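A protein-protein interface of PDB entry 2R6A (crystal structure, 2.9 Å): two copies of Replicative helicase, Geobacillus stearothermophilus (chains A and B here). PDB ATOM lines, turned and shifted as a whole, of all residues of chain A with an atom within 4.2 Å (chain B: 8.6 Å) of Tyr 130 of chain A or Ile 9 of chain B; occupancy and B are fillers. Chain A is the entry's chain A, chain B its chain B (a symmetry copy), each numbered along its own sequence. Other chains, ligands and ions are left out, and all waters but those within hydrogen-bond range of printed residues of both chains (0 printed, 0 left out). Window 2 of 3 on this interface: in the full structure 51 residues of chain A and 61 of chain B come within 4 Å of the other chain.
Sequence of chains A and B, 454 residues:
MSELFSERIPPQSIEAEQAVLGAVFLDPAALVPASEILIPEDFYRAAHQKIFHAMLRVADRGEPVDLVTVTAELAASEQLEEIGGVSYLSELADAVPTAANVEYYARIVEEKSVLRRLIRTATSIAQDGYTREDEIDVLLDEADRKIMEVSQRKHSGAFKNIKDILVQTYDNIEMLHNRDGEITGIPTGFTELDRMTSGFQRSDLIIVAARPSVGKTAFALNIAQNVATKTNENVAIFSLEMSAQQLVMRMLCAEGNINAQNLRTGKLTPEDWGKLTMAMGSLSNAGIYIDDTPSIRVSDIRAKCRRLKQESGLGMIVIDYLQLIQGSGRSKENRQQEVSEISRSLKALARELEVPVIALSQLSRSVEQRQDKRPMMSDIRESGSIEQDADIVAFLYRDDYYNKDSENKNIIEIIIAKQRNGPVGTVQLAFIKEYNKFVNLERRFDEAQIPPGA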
ATOM      1  N   ALA A 126      33.475  -2.500  26.886  1.00  0.00           N
ATOM      2  CA  ALA A 126      32.846  -3.642  27.525  1.00  0.00           C
ATOM      3  C   ALA A 126      31.329  -3.484  27.551  1.00  0.00           C
ATOM      4  O   ALA A 126      30.623  -4.395  27.136  1.00  0.00           O
ATOM      5  CB  ALA A 126      33.402  -3.864  28.922  1.00  0.00           C
ATOM      6  N   GLN A 127      30.832  -2.330  28.003  1.00  0.00           N
ATOM      7  CA  GLN A 127      29.384  -2.068  28.043  1.00  0.00           C
ATOM      8  C   GLN A 127      28.719  -2.211  26.669  1.00  0.00           C
ATOM      9  O   GLN A 127      27.738  -2.952  26.526  1.00  0.00           O
ATOM     10  CB  GLN A 127      29.071  -0.714  28.681  1.00  0.00           C
ATOM     11  CG  GLN A 127      29.146  -0.722  30.211  1.00  0.00           C
ATOM     12  CD  GLN A 127      29.272   0.683  30.835  1.00  0.00           C
ATOM     13  OE1 GLN A 127      29.676   1.648  30.175  1.00  0.00           O
ATOM     14  NE2 GLN A 127      28.940   0.788  32.120  1.00  0.00           N
ATOM     15  N   ASP A 128      29.272  -1.538  25.662  1.00  0.00           N
ATOM     16  CA  ASP A 128      28.771  -1.642  24.287  1.00  0.00           C
ATOM     17  C   ASP A 128      28.674  -3.090  23.790  1.00  0.00           C
ATOM     18  O   ASP A 128      27.806  -3.418  22.977  1.00  0.00           O
ATOM     19  CB  ASP A 128      29.635  -0.820  23.329  1.00  0.00           C
ATOM     20  CG  ASP A 128      29.285   0.656  23.338  1.00  0.00           C
ATOM     21  OD1 ASP A 128      29.366   1.279  22.259  1.00  0.00           O
ATOM     22  OD2 ASP A 128      28.922   1.192  24.407  1.00  0.00           O
ATOM     23  N   GLY A 129      29.577  -3.940  24.281  1.00  0.00           N
ATOM     24  CA  GLY A 129      29.574  -5.366  23.969  1.00  0.00           C
ATOM     25  C   GLY A 129      28.285  -6.049  24.391  1.00  0.00           C
ATOM     26  O   GLY A 129      27.773  -6.897  23.670  1.00  0.00           O
ATOM     27  N   TYR A 130      27.754  -5.681  25.556  1.00  0.00           N
ATOM     28  CA  TYR A 130      26.493  -6.253  26.031  1.00  0.00           C
ATOM     29  C   TYR A 130      25.272  -5.632  25.356  1.00  0.00           C
ATOM     30  O   TYR A 130      24.302  -6.341  25.088  1.00  0.00           O
ATOM     31  CB  TYR A 130      26.331  -6.105  27.544  1.00  0.00           C
ATOM     32  CG  TYR A 130      27.367  -6.801  28.388  1.00  0.00           C
ATOM     33  CD1 TYR A 130      28.487  -6.109  28.835  1.00  0.00           C
ATOM     34  CD2 TYR A 130      27.213  -8.134  28.771  1.00  0.00           C
ATOM     35  CE1 TYR A 130      29.442  -6.722  29.626  1.00  0.00           C
ATOM     36  CE2 TYR A 130      28.167  -8.765  29.567  1.00  0.00           C
ATOM     37  CZ  TYR A 130      29.281  -8.043  29.989  1.00  0.00           C
ATOM     38  OH  TYR A 130      30.247  -8.618  30.781  1.00  0.00           O
ATOM     39  N   THR A 131      25.310  -4.319  25.106  1.00  0.00           N
ATOM     40  CA  THR A 131      24.178  -3.606  24.496  1.00  0.00           C
ATOM     41  C   THR A 131      24.081  -3.841  22.980  1.00  0.00           C
ATOM     42  O   THR A 131      23.612  -4.897  22.547  1.00  0.00           O
ATOM     43  CB  THR A 131      24.219  -2.099  24.798  1.00  0.00           C
ATOM     44  OG1 THR A 131      24.594  -1.894  26.165  1.00  0.00           O
ATOM     45  CG2 THR A 131      22.847  -1.459  24.541  1.00  0.00           C
ATOM     46  N   GLU A 133      24.237  -5.138  19.589  1.00  0.00           N
ATOM     47  CA  GLU A 133      24.590  -6.534  19.338  1.00  0.00           C
ATOM     48  C   GLU A 133      23.999  -7.340  18.127  1.00  0.00           C
ATOM     49  O   GLU A 133      24.017  -8.574  18.213  1.00  0.00           O
ATOM     50  CB  GLU A 133      24.242  -7.287  20.636  1.00  0.00           C
ATOM     51  CG  GLU A 133      25.166  -8.413  21.060  1.00  0.00           C
ATOM     52  CD  GLU A 133      24.626  -9.172  22.264  1.00  0.00           C
ATOM     53  OE1 GLU A 133      23.683  -9.979  22.099  1.00  0.00           O
ATOM     54  OE2 GLU A 133      25.155  -8.964  23.374  1.00  0.00           O
ATOM     55  N   ILE B   9      24.718 -10.332  31.427  1.00  0.00           N
ATOM     56  CA  ILE B   9      24.545 -11.636  30.712  1.00  0.00           C
ATOM     57  C   ILE B   9      25.442 -11.701  29.461  1.00  0.00           C
ATOM     58  O   ILE B   9      25.252 -10.923  28.516  1.00  0.00           O
ATOM     59  CB  ILE B   9      23.061 -11.885  30.319  1.00  0.00           C
ATOM     60  CG1 ILE B   9      22.164 -11.856  31.559  1.00  0.00           C
ATOM     61  CG2 ILE B   9      22.914 -13.201  29.548  1.00  0.00           C
ATOM     62  CD1 ILE B   9      20.681 -11.851  31.243  1.00  0.00           C
ATOM     63  N   PRO B  10      26.402 -12.648  29.437  1.00  0.00           N
ATOM     64  CA  PRO B  10      27.350 -12.664  28.324  1.00  0.00           C
ATOM     65  C   PRO B  10      26.669 -13.020  27.000  1.00  0.00           C
ATOM     66  O   PRO B  10      25.887 -13.972  26.957  1.00  0.00           O
ATOM     67  CB  PRO B  10      28.370 -13.745  28.729  1.00  0.00           C
ATOM     68  CG  PRO B  10      28.091 -14.052  30.177  1.00  0.00           C
ATOM     69  CD  PRO B  10      26.648 -13.744  30.394  1.00  0.00           C
ATOM     70  N   PRO B  11      26.946 -12.247  25.927  1.00  0.00           N
ATOM     71  CA  PRO B  11      26.363 -12.506  24.610  1.00  0.00           C
ATOM     72  C   PRO B  11      26.450 -13.984  24.250  1.00  0.00           C
ATOM     73  O   PRO B  11      27.528 -14.583  24.329  1.00  0.00           O
ATOM     74  CB  PRO B  11      27.238 -11.675  23.674  1.00  0.00           C
ATOM     75  CG  PRO B  11      27.696 -10.552  24.506  1.00  0.00           C
ATOM     76  CD  PRO B  11      27.826 -11.065  25.912  1.00  0.00           C
ATOM     77  N   GLN B  12      25.315 -14.558  23.862  1.00  0.00           N
ATOM     78  CA  GLN B  12      25.221 -15.986  23.575  1.00  0.00           C
ATOM     79  C   GLN B  12      23.998 -16.311  22.717  1.00  0.00           C
ATOM     80  O   GLN B  12      23.079 -15.498  22.601  1.00  0.00           O
ATOM     81  CB  GLN B  12      25.112 -16.758  24.896  1.00  0.00           C
ATOM     82  CG  GLN B  12      23.751 -16.635  25.578  1.00  0.00           C
ATOM     83  CD  GLN B  12      23.799 -16.989  27.046  1.00  0.00           C
ATOM     84  OE1 GLN B  12      24.503 -16.348  27.826  1.00  0.00           O
ATOM     85  NE2 GLN B  12      23.032 -18.004  27.439  1.00  0.00           N
ATOM     86  N   TYR B  44      29.244 -21.121  24.077  1.00  0.00           N
ATOM     87  CA  TYR B  44      29.208 -20.535  25.408  1.00  0.00           C
ATOM     88  C   TYR B  44      29.058 -21.568  26.516  1.00  0.00           C
ATOM     89  O   TYR B  44      29.667 -21.412  27.578  1.00  0.00           O
ATOM     90  CB  TYR B  44      28.111 -19.473  25.528  1.00  0.00           C
ATOM     91  CG  TYR B  44      27.999 -18.910  26.924  1.00  0.00           C
ATOM     92  CD1 TYR B  44      28.967 -18.040  27.420  1.00  0.00           C
ATOM     93  CD2 TYR B  44      26.937 -19.252  27.751  1.00  0.00           C
ATOM     94  CE1 TYR B  44      28.882 -17.527  28.698  1.00  0.00           C
ATOM     95  CE2 TYR B  44      26.841 -18.745  29.032  1.00  0.00           C
ATOM     96  CZ  TYR B  44      27.817 -17.886  29.494  1.00  0.00           C
ATOM     97  OH  TYR B  44      27.739 -17.382  30.755  1.00  0.00           O
ATOM     98  N   LYS B 112      28.673 -14.079  18.710  1.00  0.00           N
ATOM     99  CA  LYS B 112      28.546 -13.992  20.163  1.00  0.00           C
ATOM    100  C   LYS B 112      29.888 -14.261  20.840  1.00  0.00           C
ATOM    101  O   LYS B 112      30.228 -13.627  21.842  1.00  0.00           O
ATOM    102  CB  LYS B 112      27.491 -14.979  20.671  1.00  0.00           C
ATOM    103  CG  LYS B 112      26.097 -14.772  20.085  1.00  0.00           C
ATOM    104  CD  LYS B 112      25.464 -13.464  20.519  1.00  0.00           C
ATOM    105  CE  LYS B 112      24.174 -13.222  19.763  1.00  0.00           C
ATOM    106  NZ  LYS B 112      23.602 -11.887  20.088  1.00  0.00           N
ATOM    107  N   LEU B 115      32.120 -11.148  20.477  1.00  0.00           N
ATOM    108  CA  LEU B 115      31.657 -10.165  21.457  1.00  0.00           C
ATOM    109  C   LEU B 115      32.083 -10.501  22.883  1.00  0.00           C
ATOM    110  O   LEU B 115      32.436  -9.606  23.653  1.00  0.00           O
ATOM    111  CB  LEU B 115      30.142  -9.984  21.386  1.00  0.00           C
ATOM    112  CG  LEU B 115      29.650  -9.221  20.160  1.00  0.00           C
ATOM    113  CD1 LEU B 115      28.186  -9.473  19.925  1.00  0.00           C
ATOM    114  CD2 LEU B 115      29.921  -7.736  20.306  1.00  0.00           C
ATOM    115  N   ARG B 116      32.055 -11.779  23.241  1.00  0.00           N
ATOM    116  CA  ARG B 116      32.527 -12.166  24.563  1.00  0.00           C
ATOM    117  C   ARG B 116      34.008 -11.809  24.685  1.00  0.00           C
ATOM    118  O   ARG B 116      34.420 -11.190  25.665  1.00  0.00           O
ATOM    119  CB  ARG B 116      32.249 -13.647  24.866  1.00  0.00           C
ATOM    120  CG  ARG B 116      30.766 -13.935  25.145  1.00  0.00           C
ATOM    121  CD  ARG B 116      30.531 -15.273  25.863  1.00  0.00           C
ATOM    122  NE  ARG B 116      31.104 -16.417  25.155  1.00  0.00           N
ATOM    123  CZ  ARG B 116      30.567 -16.984  24.072  1.00  0.00           C
ATOM    124  NH1 ARG B 116      29.434 -16.513  23.549  1.00  0.00           N
ATOM    125  NH2 ARG B 116      31.175 -18.024  23.503  1.00  0.00           N
ATOM    126  N   LEU B 118      35.687  -9.584  23.017  1.00  0.00           N
ATOM    127  CA  LEU B 118      35.774  -8.136  23.062  1.00  0.00           C
ATOM    128  C   LEU B 118      35.597  -7.667  24.507  1.00  0.00           C
ATOM    129  O   LEU B 118      36.415  -6.908  25.030  1.00  0.00           O
ATOM    130  CB  LEU B 118      34.699  -7.510  22.169  1.00  0.00           C
ATOM    131  CG  LEU B 118      34.617  -5.980  22.130  1.00  0.00           C
ATOM    132  CD1 LEU B 118      35.880  -5.419  21.524  1.00  0.00           C
ATOM    133  CD2 LEU B 118      33.403  -5.506  21.354  1.00  0.00           C
ATOM    134  N   ILE B 119      34.527  -8.145  25.138  1.00  0.00           N
ATOM    135  CA  ILE B 119      34.208  -7.811  26.517  1.00  0.00           C
ATOM    136  C   ILE B 119      35.332  -8.231  27.460  1.00  0.00           C
ATOM    137  O   ILE B 119      35.763  -7.444  28.298  1.00  0.00           O
ATOM    138  CB  ILE B 119      32.838  -8.419  26.935  1.00  0.00           C
ATOM    139  CG1 ILE B 119      31.711  -7.714  26.170  1.00  0.00           C
ATOM    140  CG2 ILE B 119      32.601  -8.277  28.425  1.00  0.00           C
ATOM    141  CD1 ILE B 119      30.380  -8.424  26.195  1.00  0.00           C
ATOM    142  N   ARG B 120      35.826  -9.452  27.302  1.00  0.00           N
ATOM    143  CA  ARG B 120      36.879  -9.971  28.172  1.00  0.00           C
ATOM    144  C   ARG B 120      38.152  -9.138  28.064  1.00  0.00           C
ATOM    145  O   ARG B 120      38.798  -8.857  29.077  1.00  0.00           O
ATOM    146  CB  ARG B 120      37.173 -11.427  27.828  1.00  0.00           C
ATOM    147  CG  ARG B 120      38.104 -12.167  28.786  1.00  0.00           C
ATOM    148  CD  ARG B 120      38.605 -13.434  28.097  1.00  0.00           C
ATOM    149  NE  ARG B 120      37.517 -14.072  27.353  1.00  0.00           N
ATOM    150  CZ  ARG B 120      37.639 -14.620  26.146  1.00  0.00           C
ATOM    151  NH1 ARG B 120      38.811 -14.605  25.512  1.00  0.00           N
ATOM    152  NH2 ARG B 120      36.575 -15.157  25.561  1.00  0.00           N
ATOM    153  N   ALA B 122      38.462  -5.895  26.989  1.00  0.00           N
ATOM    154  CA  ALA B 122      38.212  -4.560  27.510  1.00  0.00           C
ATOM    155  C   ALA B 122      38.143  -4.520  29.038  1.00  0.00           C
ATOM    156  O   ALA B 122      38.689  -3.604  29.663  1.00  0.00           O
ATOM    157  CB  ALA B 122      36.954  -3.972  26.892  1.00  0.00           C
ATOM    158  N   THR B 123      37.485  -5.508  29.639  1.00  0.00           N
ATOM    159  CA  THR B 123      37.380  -5.578  31.093  1.00  0.00           C
ATOM    160  C   THR B 123      38.771  -5.696  31.701  1.00  0.00           C
ATOM    161  O   THR B 123      39.105  -5.009  32.674  1.00  0.00           O
ATOM    162  CB  THR B 123      36.508  -6.768  31.520  1.00  0.00           C
ATOM    163  OG1 THR B 123      35.182  -6.562  31.030  1.00  0.00           O
ATOM    164  CG2 THR B 123      36.464  -6.927  33.035  1.00  0.00           C
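The side-chain carboxylate (OE1) of Glu 133 of chain A lies within salt-bridge range of the side-chain amino group (NZ) of Lys 112 of chain B.
The backbone carbonyl oxygen (O) of Pro 11 of chain B sits at hydrogen-bond distance from the guanidinium group (NH1) of Arg 116 of chain B, at 2.8 Å.
O of Lys 112 of chain B sits close to NH1 of Arg 116 of chain B, 3.4 Å away.
The backbone carbonyl oxygen of Ile 119 of chain B is in hydrogen-bond range of the side-chain hydroxyl of Thr 123 of chain B (2.9 Å).
Ile 119 of chain B touches Ala 126 of chain A.
Ala 122 of chain B touches Ala 126 of chain A (CB to N, 3.8 Å).
Ala 126 of chain A touches Thr 123 of chain B.
Pro 11 of chain B touches Gly 129 of chain A (CG to O, 3.8 Å).
Gly 129 of chain A touches Ile 119 of chain B (C to CD1, 3.6 Å).
Tyr 130 of chain A touches Ile 9 of chain B (CD2 to O, 3.4 Å).
Ile 119 of chain B touches Tyr 130 of chain A (CG2 to OH, 3.3 Å).
OE2 of Glu 133 of chain A touches CG of Pro 11 of chain B, at 3.2 Å.
Glu 133 of chain A touches Leu 115 of chain B (CG to CD1, 3.4 Å).
Printed residues of chain B within 4 Å of Ala 126 of chain A: Ile 119, Ala 122 and Thr 123.
Of chain B, only Pro 11 (3.8 Å) and Ile 119 (3.6 Å) come within 4 Å of Gly 129 of chain A.
Tyr 130 of chain A touches two residues of chain B.
Ile 9 of chain B touches just one residue of chain A: Tyr 130 (3.4 Å).
Of the printed residues of chain A, Pro 11 of chain B touches Gly 129 (3.8 Å) and Glu 133 (3.2 Å).
Gln 12 of chain B touches none of the printed residues of chain A.
Of the printed residues of chain A, Ile 119 of chain B touches Ala 126 (3.6 Å), Gly 129 (3.6 Å) and Tyr 130 (3.3 Å).
Of the printed residues of chain A, Ala 122 of chain B touches Ala 126.
Of the 13 printed residues of chain B, 7 touch a printed residue of chain A.
No position is printed for both chains.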
